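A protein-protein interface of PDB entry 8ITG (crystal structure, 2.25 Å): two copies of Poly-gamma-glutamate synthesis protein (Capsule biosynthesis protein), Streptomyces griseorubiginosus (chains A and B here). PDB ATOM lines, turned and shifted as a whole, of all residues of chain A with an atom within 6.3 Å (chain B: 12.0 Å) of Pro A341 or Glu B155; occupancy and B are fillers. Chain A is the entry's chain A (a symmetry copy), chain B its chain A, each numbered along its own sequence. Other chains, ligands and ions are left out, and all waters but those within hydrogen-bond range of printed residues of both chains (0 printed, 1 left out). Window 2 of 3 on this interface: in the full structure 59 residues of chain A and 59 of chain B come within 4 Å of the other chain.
The backbone carbonyl oxygen (O) of Val A325 lies within hydrogen-bond range of the side-chain hydroxyl (OG) of Ser B153, at 2.7 Å.
The side-chain hydroxyl (OH) of Tyr A330 lies within hydrogen-bond range of the side-chain carboxylate (OE1) of Glu B155 (3.0 Å).
OG of Ser B153 lies within hydrogen-bond range of N of Leu B156.
The backbone NH (N) of Glu B155 lies close to the side-chain hydroxyl (OG) of Ser B153 (3.2 Å).
The side-chain hydroxyl (OH) of Tyr A330 lies close to the backbone carbonyl oxygen (O) of Leu A339, at 3.4 Å.
Glu B155 touches Asp A323.
CA of Arg A324 touches CB of Glu B155, 3.97 Å away.
CD1 of Leu B156 touches O of Arg A324, at 3.5 Å.
O of Val A325 touches OE1 of Glu B155, at 3.6 Å.
CD1 of Leu B156 touches C of Val A325 (3.7 Å).
C of Ser A326 touches CB of Ser B153 (3.7 Å).
Leu B156 touches Ser A326.
Pro A341 touches Glu B155.
Glu B155 touches just these residues of chain A: Asp A323 (3.1 Å), Arg A324 (3.97 Å), Val A325 (3.6 Å), Tyr A330 (3.0 Å) and Pro A341 (3.7 Å).
Val A325 touches just these residues of chain B: Ser B153, Glu B155 and Leu B156.
No residue of chain B comes within 4 Å of Leu A339.
No residue of chain B comes within 4 Å of Gly A342.
No residue of chain B comes within 4 Å of Tyr A344.
No residue of chain B comes within 4 Å of Tyr A345.
Of the printed residues of chain B, Ser A326 touches Ser B153 and Leu B156.
Of the printed residues of chain B, Tyr A330 touches Glu B155.
Of the printed residues of chain A, Ser B153 touches Val A325 and Ser A326.
Of the printed residues of chain A, Leu B156 touches Arg A324 (3.5 Å), Val A325 (3.7 Å) and Ser A326 (3.6 Å).
Arg A343 touches none of the printed residues of chain B.
Asp B151 touches none of the printed residues of chain A.
Printed residues of chain B that touch a printed residue of chain A: Ser B153, Glu B155 and Leu B156.
Hydrophobic or aromatic side chains of chain B within 4 Å of the printed part of chain A: Leu B156.
Along chain B the printed residues that touch a printed residue of chain A span positions 153 to 156.
Among the printed residues, no Asp or Glu carboxylate lies within 4 Å of a Lys or Arg side-chain nitrogen of the other chain.
No position is printed for both chains.
Of the 10 pairs that touch across the chains among the printed residues, none has its exchanged pair printed and touching as well.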
ATOM      1  N   GLU A 320     -31.672 -11.696 -12.752  1.00  0.00           N
ATOM      2  CA  GLU A 320     -30.894 -10.614 -13.341  1.00  0.00           C
ATOM      3  C   GLU A 320     -31.663  -9.306 -13.453  1.00  0.00           C
ATOM      4  O   GLU A 320     -31.071  -8.301 -13.865  1.00  0.00           O
ATOM      5  CB  GLU A 320     -30.385 -11.036 -14.719  1.00  0.00           C
ATOM      6  CG  GLU A 320     -29.339 -12.138 -14.671  1.00  0.00           C
ATOM      7  CD  GLU A 320     -28.947 -12.628 -16.050  1.00  0.00           C
ATOM      8  OE1 GLU A 320     -29.820 -13.173 -16.759  1.00  0.00           O
ATOM      9  OE2 GLU A 320     -27.768 -12.459 -16.427  1.00  0.00           O
ATOM     10  N   THR A 322     -33.320  -8.013 -10.696  1.00  0.00           N
ATOM     11  CA  THR A 322     -33.498  -7.463  -9.359  1.00  0.00           C
ATOM     12  C   THR A 322     -32.902  -6.062  -9.283  1.00  0.00           C
ATOM     13  O   THR A 322     -31.885  -5.759  -9.916  1.00  0.00           O
ATOM     14  CB  THR A 322     -32.864  -8.377  -8.301  1.00  0.00           C
ATOM     15  OG1 THR A 322     -33.374  -8.035  -7.007  1.00  0.00           O
ATOM     16  CG2 THR A 322     -31.359  -8.230  -8.274  1.00  0.00           C
ATOM     17  N   ASP A 323     -33.570  -5.191  -8.533  1.00  0.00           N
ATOM     18  CA  ASP A 323     -33.113  -3.826  -8.328  1.00  0.00           C
ATOM     19  C   ASP A 323     -32.521  -3.618  -6.942  1.00  0.00           C
ATOM     20  O   ASP A 323     -32.306  -2.472  -6.536  1.00  0.00           O
ATOM     21  CB  ASP A 323     -34.267  -2.848  -8.560  1.00  0.00           C
ATOM     22  CG  ASP A 323     -33.897  -1.719  -9.504  1.00  0.00           C
ATOM     23  OD1 ASP A 323     -32.717  -1.638  -9.910  1.00  0.00           O
ATOM     24  OD2 ASP A 323     -34.789  -0.915  -9.845  1.00  0.00           O
ATOM     25  N   ARG A 324     -32.258  -4.698  -6.205  1.00  0.00           N
ATOM     26  CA  ARG A 324     -31.767  -4.629  -4.828  1.00  0.00           C
ATOM     27  C   ARG A 324     -30.568  -5.566  -4.699  1.00  0.00           C
ATOM     28  O   ARG A 324     -30.717  -6.736  -4.335  1.00  0.00           O
ATOM     29  CB  ARG A 324     -32.878  -4.983  -3.836  1.00  0.00           C
ATOM     30  CG  ARG A 324     -34.209  -4.298  -4.123  1.00  0.00           C
ATOM     31  CD  ARG A 324     -35.049  -4.139  -2.867  1.00  0.00           C
ATOM     32  NE  ARG A 324     -36.382  -3.619  -3.163  1.00  0.00           N
ATOM     33  CZ  ARG A 324     -37.219  -3.142  -2.247  1.00  0.00           C
ATOM     34  NH1 ARG A 324     -36.861  -3.108  -0.969  1.00  0.00           N
ATOM     35  NH2 ARG A 324     -38.413  -2.691  -2.607  1.00  0.00           N
ATOM     36  N   VAL A 325     -29.379  -5.045  -4.994  1.00  0.00           N
ATOM     37  CA  VAL A 325     -28.129  -5.797  -4.915  1.00  0.00           C
ATOM     38  C   VAL A 325     -27.337  -5.283  -3.718  1.00  0.00           C
ATOM     39  O   VAL A 325     -27.154  -4.069  -3.562  1.00  0.00           O
ATOM     40  CB  VAL A 325     -27.318  -5.672  -6.217  1.00  0.00           C
ATOM     41  CG1 VAL A 325     -25.948  -6.321  -6.067  1.00  0.00           C
ATOM     42  CG2 VAL A 325     -28.083  -6.297  -7.377  1.00  0.00           C
ATOM     43  N   SER A 326     -26.866  -6.203  -2.880  1.00  0.00           N
ATOM     44  CA  SER A 326     -26.176  -5.822  -1.657  1.00  0.00           C
ATOM     45  C   SER A 326     -24.719  -5.458  -1.944  1.00  0.00           C
ATOM     46  O   SER A 326     -24.175  -5.736  -3.017  1.00  0.00           O
ATOM     47  CB  SER A 326     -26.244  -6.947  -0.625  1.00  0.00           C
ATOM     48  OG  SER A 326     -25.340  -7.990  -0.942  1.00  0.00           O
ATOM     49  N   TYR A 330     -22.102  -6.819  -4.817  1.00  0.00           N
ATOM     50  CA  TYR A 330     -21.347  -5.967  -5.733  1.00  0.00           C
ATOM     51  C   TYR A 330     -19.854  -6.259  -5.676  1.00  0.00           C
ATOM     52  O   TYR A 330     -19.160  -6.143  -6.695  1.00  0.00           O
ATOM     53  CB  TYR A 330     -21.591  -4.490  -5.418  1.00  0.00           C
ATOM     54  CG  TYR A 330     -22.836  -3.900  -6.044  1.00  0.00           C
ATOM     55  CD1 TYR A 330     -22.976  -3.829  -7.424  1.00  0.00           C
ATOM     56  CD2 TYR A 330     -23.861  -3.392  -5.254  1.00  0.00           C
ATOM     57  CE1 TYR A 330     -24.108  -3.285  -8.002  1.00  0.00           C
ATOM     58  CE2 TYR A 330     -24.994  -2.845  -5.821  1.00  0.00           C
ATOM     59  CZ  TYR A 330     -25.113  -2.794  -7.196  1.00  0.00           C
ATOM     60  OH  TYR A 330     -26.242  -2.250  -7.766  1.00  0.00           O
ATOM     61  N   LEU A 339     -21.274   0.395  -9.848  1.00  0.00           N
ATOM     62  CA  LEU A 339     -22.087  -0.367 -10.786  1.00  0.00           C
ATOM     63  C   LEU A 339     -23.573  -0.217 -10.486  1.00  0.00           C
ATOM     64  O   LEU A 339     -23.990  -0.217  -9.325  1.00  0.00           O
ATOM     65  CB  LEU A 339     -21.717  -1.851 -10.755  1.00  0.00           C
ATOM     66  CG  LEU A 339     -20.392  -2.249 -11.401  1.00  0.00           C
ATOM     67  CD1 LEU A 339     -20.292  -3.763 -11.508  1.00  0.00           C
ATOM     68  CD2 LEU A 339     -20.244  -1.596 -12.766  1.00  0.00           C
ATOM     69  N   THR A 340     -24.361  -0.095 -11.546  1.00  0.00           N
ATOM     70  CA  THR A 340     -25.800  -0.245 -11.460  1.00  0.00           C
ATOM     71  C   THR A 340     -26.154  -1.731 -11.461  1.00  0.00           C
ATOM     72  O   THR A 340     -25.345  -2.565 -11.881  1.00  0.00           O
ATOM     73  CB  THR A 340     -26.470   0.477 -12.628  1.00  0.00           C
ATOM     74  OG1 THR A 340     -26.013  -0.084 -13.865  1.00  0.00           O
ATOM     75  CG2 THR A 340     -26.141   1.965 -12.596  1.00  0.00           C
ATOM     76  N   PRO A 341     -27.347  -2.095 -10.976  1.00  0.00           N
ATOM     77  CA  PRO A 341     -27.681  -3.532 -10.878  1.00  0.00           C
ATOM     78  C   PRO A 341     -27.574  -4.286 -12.196  1.00  0.00           C
ATOM     79  O   PRO A 341     -26.968  -5.366 -12.239  1.00  0.00           O
ATOM     80  CB  PRO A 341     -29.120  -3.515 -10.342  1.00  0.00           C
ATOM     81  CG  PRO A 341     -29.224  -2.230  -9.597  1.00  0.00           C
ATOM     82  CD  PRO A 341     -28.385  -1.247 -10.359  1.00  0.00           C
ATOM     83  N   GLY A 342     -28.149  -3.749 -13.276  1.00  0.00           N
ATOM     84  CA  GLY A 342     -28.114  -4.453 -14.549  1.00  0.00           C
ATOM     85  C   GLY A 342     -26.705  -4.649 -15.077  1.00  0.00           C
ATOM     86  O   GLY A 342     -26.361  -5.728 -15.567  1.00  0.00           O
ATOM     87  N   ARG A 343     -25.871  -3.607 -14.991  1.00  0.00           N
ATOM     88  CA  ARG A 343     -24.473  -3.749 -15.384  1.00  0.00           C
ATOM     89  C   ARG A 343     -23.741  -4.746 -14.497  1.00  0.00           C
ATOM     90  O   ARG A 343     -22.834  -5.444 -14.964  1.00  0.00           O
ATOM     91  CB  ARG A 343     -23.767  -2.394 -15.336  1.00  0.00           C
ATOM     92  CG  ARG A 343     -24.157  -1.431 -16.442  1.00  0.00           C
ATOM     93  CD  ARG A 343     -23.309  -0.171 -16.357  1.00  0.00           C
ATOM     94  NE  ARG A 343     -23.623   0.794 -17.406  1.00  0.00           N
ATOM     95  CZ  ARG A 343     -24.549   1.741 -17.296  1.00  0.00           C
ATOM     96  NH1 ARG A 343     -25.262   1.847 -16.183  1.00  0.00           N
ATOM     97  NH2 ARG A 343     -24.763   2.581 -18.300  1.00  0.00           N
ATOM     98  N   TYR A 344     -24.116  -4.822 -13.218  1.00  0.00           N
ATOM     99  CA  TYR A 344     -23.495  -5.789 -12.318  1.00  0.00           C
ATOM    100  C   TYR A 344     -23.784  -7.219 -12.759  1.00  0.00           C
ATOM    101  O   TYR A 344     -22.884  -8.066 -12.773  1.00  0.00           O
ATOM    102  CB  TYR A 344     -23.983  -5.550 -10.888  1.00  0.00           C
ATOM    103  CG  TYR A 344     -23.921  -6.768  -9.996  1.00  0.00           C
ATOM    104  CD1 TYR A 344     -22.736  -7.136  -9.370  1.00  0.00           C
ATOM    105  CD2 TYR A 344     -25.050  -7.546  -9.771  1.00  0.00           C
ATOM    106  CE1 TYR A 344     -22.677  -8.247  -8.550  1.00  0.00           C
ATOM    107  CE2 TYR A 344     -25.001  -8.659  -8.955  1.00  0.00           C
ATOM    108  CZ  TYR A 344     -23.811  -9.004  -8.345  1.00  0.00           C
ATOM    109  OH  TYR A 344     -23.762 -10.112  -7.530  1.00  0.00           O
ATOM    110  N   TYR A 345     -25.036  -7.507 -13.121  1.00  0.00           N
ATOM    111  CA  TYR A 345     -25.368  -8.850 -13.584  1.00  0.00           C
ATOM    112  C   TYR A 345     -24.761  -9.142 -14.947  1.00  0.00           C
ATOM    113  O   TYR A 345     -24.445 -10.300 -15.247  1.00  0.00           O
ATOM    114  CB  TYR A 345     -26.882  -9.040 -13.616  1.00  0.00           C
ATOM    115  CG  TYR A 345     -27.441  -9.338 -12.251  1.00  0.00           C
ATOM    116  CD1 TYR A 345     -27.327 -10.609 -11.701  1.00  0.00           C
ATOM    117  CD2 TYR A 345     -28.058  -8.348 -11.498  1.00  0.00           C
ATOM    118  CE1 TYR A 345     -27.821 -10.891 -10.448  1.00  0.00           C
ATOM    119  CE2 TYR A 345     -28.556  -8.620 -10.240  1.00  0.00           C
ATOM    120  CZ  TYR A 345     -28.435  -9.894  -9.720  1.00  0.00           C
ATOM    121  OH  TYR A 345     -28.928 -10.184  -8.470  1.00  0.00           O
ATOM    122  N   ASP A 346     -24.583  -8.116 -15.781  1.00  0.00           N
ATOM    123  CA  ASP A 346     -23.921  -8.331 -17.062  1.00  0.00           C
ATOM    124  C   ASP A 346     -22.462  -8.722 -16.860  1.00  0.00           C
ATOM    125  O   ASP A 346     -21.957  -9.631 -17.528  1.00  0.00           O
ATOM    126  CB  ASP A 346     -24.036  -7.078 -17.930  1.00  0.00           C
ATOM    127  CG  ASP A 346     -23.656  -7.335 -19.374  1.00  0.00           C
ATOM    128  OD1 ASP A 346     -24.346  -8.141 -20.035  1.00  0.00           O
ATOM    129  OD2 ASP A 346     -22.671  -6.732 -19.850  1.00  0.00           O
ATOM    130  N   ALA B 150     -21.800  -5.430   7.610  1.00  0.00           N
ATOM    131  CA  ALA B 150     -21.745  -5.134   6.187  1.00  0.00           C
ATOM    132  C   ALA B 150     -22.085  -3.670   5.966  1.00  0.00           C
ATOM    133  O   ALA B 150     -22.936  -3.109   6.661  1.00  0.00           O
ATOM    134  CB  ALA B 150     -22.707  -6.028   5.385  1.00  0.00           C
ATOM    135  N   ASP B 151     -21.402  -3.054   5.007  1.00  0.00           N
ATOM    136  CA  ASP B 151     -21.682  -1.679   4.629  1.00  0.00           C
ATOM    137  C   ASP B 151     -22.874  -1.625   3.675  1.00  0.00           C
ATOM    138  O   ASP B 151     -23.222  -2.627   3.047  1.00  0.00           O
ATOM    139  CB  ASP B 151     -20.447  -1.058   3.985  1.00  0.00           C
ATOM    140  CG  ASP B 151     -19.548  -0.376   4.998  1.00  0.00           C
ATOM    141  OD1 ASP B 151     -20.058   0.036   6.063  1.00  0.00           O
ATOM    142  OD2 ASP B 151     -18.336  -0.248   4.726  1.00  0.00           O
ATOM    143  N   PRO B 152     -23.534  -0.472   3.562  1.00  0.00           N
ATOM    144  CA  PRO B 152     -24.679  -0.379   2.653  1.00  0.00           C
ATOM    145  C   PRO B 152     -24.236  -0.309   1.202  1.00  0.00           C
ATOM    146  O   PRO B 152     -23.099   0.038   0.878  1.00  0.00           O
ATOM    147  CB  PRO B 152     -25.380   0.921   3.073  1.00  0.00           C
ATOM    148  CG  PRO B 152     -24.706   1.357   4.353  1.00  0.00           C
ATOM    149  CD  PRO B 152     -23.335   0.780   4.311  1.00  0.00           C
ATOM    150  N   SER B 153     -25.164  -0.654   0.329  1.00  0.00           N
ATOM    151  CA  SER B 153     -25.052  -0.488  -1.106  1.00  0.00           C
ATOM    152  C   SER B 153     -25.995   0.627  -1.545  1.00  0.00           C
ATOM    153  O   SER B 153     -26.802   1.119  -0.749  1.00  0.00           O
ATOM    154  CB  SER B 153     -25.396  -1.804  -1.819  1.00  0.00           C
ATOM    155  OG  SER B 153     -26.798  -1.981  -1.932  1.00  0.00           O
ATOM    156  N   PRO B 154     -25.905   1.075  -2.800  1.00  0.00           N
ATOM    157  CA  PRO B 154     -26.854   2.102  -3.261  1.00  0.00           C
ATOM    158  C   PRO B 154     -28.316   1.719  -3.077  1.00  0.00           C
ATOM    159  O   PRO B 154     -29.163   2.610  -2.939  1.00  0.00           O
ATOM    160  CB  PRO B 154     -26.486   2.263  -4.741  1.00  0.00           C
ATOM    161  CG  PRO B 154     -25.029   1.958  -4.781  1.00  0.00           C
ATOM    162  CD  PRO B 154     -24.825   0.854  -3.781  1.00  0.00           C
ATOM    163  N   GLU B 155     -28.636   0.421  -3.039  1.00  0.00           N
ATOM    164  CA  GLU B 155     -30.019  -0.034  -2.973  1.00  0.00           C
ATOM    165  C   GLU B 155     -30.402  -0.719  -1.669  1.00  0.00           C
ATOM    166  O   GLU B 155     -31.592  -0.756  -1.340  1.00  0.00           O
ATOM    167  CB  GLU B 155     -30.321  -1.004  -4.124  1.00  0.00           C
ATOM    168  CG  GLU B 155     -30.236  -0.378  -5.493  1.00  0.00           C
ATOM    169  CD  GLU B 155     -28.841  -0.422  -6.081  1.00  0.00           C
ATOM    170  OE1 GLU B 155     -28.018  -1.233  -5.602  1.00  0.00           O
ATOM    171  OE2 GLU B 155     -28.573   0.350  -7.027  1.00  0.00           O
ATOM    172  N   LEU B 156     -29.447  -1.278  -0.936  1.00  0.00           N
ATOM    173  CA  LEU B 156     -29.786  -2.010   0.272  1.00  0.00           C
ATOM    174  C   LEU B 156     -29.004  -1.462   1.454  1.00  0.00           C
ATOM    175  O   LEU B 156     -27.882  -0.974   1.293  1.00  0.00           O
ATOM    176  CB  LEU B 156     -29.495  -3.510   0.112  1.00  0.00           C
ATOM    177  CG  LEU B 156     -30.421  -4.272  -0.841  1.00  0.00           C
ATOM    178  CD1 LEU B 156     -29.896  -5.678  -1.085  1.00  0.00           C
ATOM    179  CD2 LEU B 156     -31.844  -4.315  -0.295  1.00  0.00           C
ATOM    180  N   PRO B 157     -29.577  -1.525   2.652  1.00  0.00           N
ATOM    181  CA  PRO B 157     -28.839  -1.099   3.844  1.00  0.00           C
ATOM    182  C   PRO B 157     -27.684  -2.042   4.137  1.00  0.00           C
ATOM    183  O   PRO B 157     -27.504  -3.088   3.508  1.00  0.00           O
ATOM    184  CB  PRO B 157     -29.894  -1.153   4.952  1.00  0.00           C
ATOM    185  CG  PRO B 157     -30.888  -2.170   4.468  1.00  0.00           C
ATOM    186  CD  PRO B 157     -30.944  -1.972   2.977  1.00  0.00           C
ATOM    187  N   GLY B 158     -26.887  -1.652   5.125  1.00  0.00           N
ATOM    188  CA  GLY B 158     -25.857  -2.521   5.641  1.00  0.00           C
ATOM    189  C   GLY B 158     -26.455  -3.619   6.498  1.00  0.00           C
ATOM    190  O   GLY B 158     -27.664  -3.857   6.515  1.00  0.00           O
ATOM    191  N   ARG B 159     -25.578  -4.300   7.227  1.00  0.00           N
ATOM    192  CA  ARG B 159     -25.993  -5.323   8.170  1.00  0.00           C
ATOM    193  C   ARG B 159     -25.263  -5.089   9.486  1.00  0.00           C
ATOM    194  O   ARG B 159     -24.024  -4.972   9.497  1.00  0.00           O
ATOM    195  CB  ARG B 159     -25.702  -6.737   7.642  1.00  0.00           C
ATOM    196  CG  ARG B 159     -26.080  -7.839   8.626  1.00  0.00           C
ATOM    197  CD  ARG B 159     -25.744  -9.223   8.099  1.00  0.00           C
ATOM    198  NE  ARG B 159     -24.307  -9.411   7.914  1.00  0.00           N
ATOM    199  CZ  ARG B 159     -23.707  -9.474   6.729  1.00  0.00           C
ATOM    200  NH1 ARG B 159     -24.419  -9.375   5.612  1.00  0.00           N
ATOM    201  NH2 ARG B 159     -22.394  -9.647   6.662  1.00  0.00           N
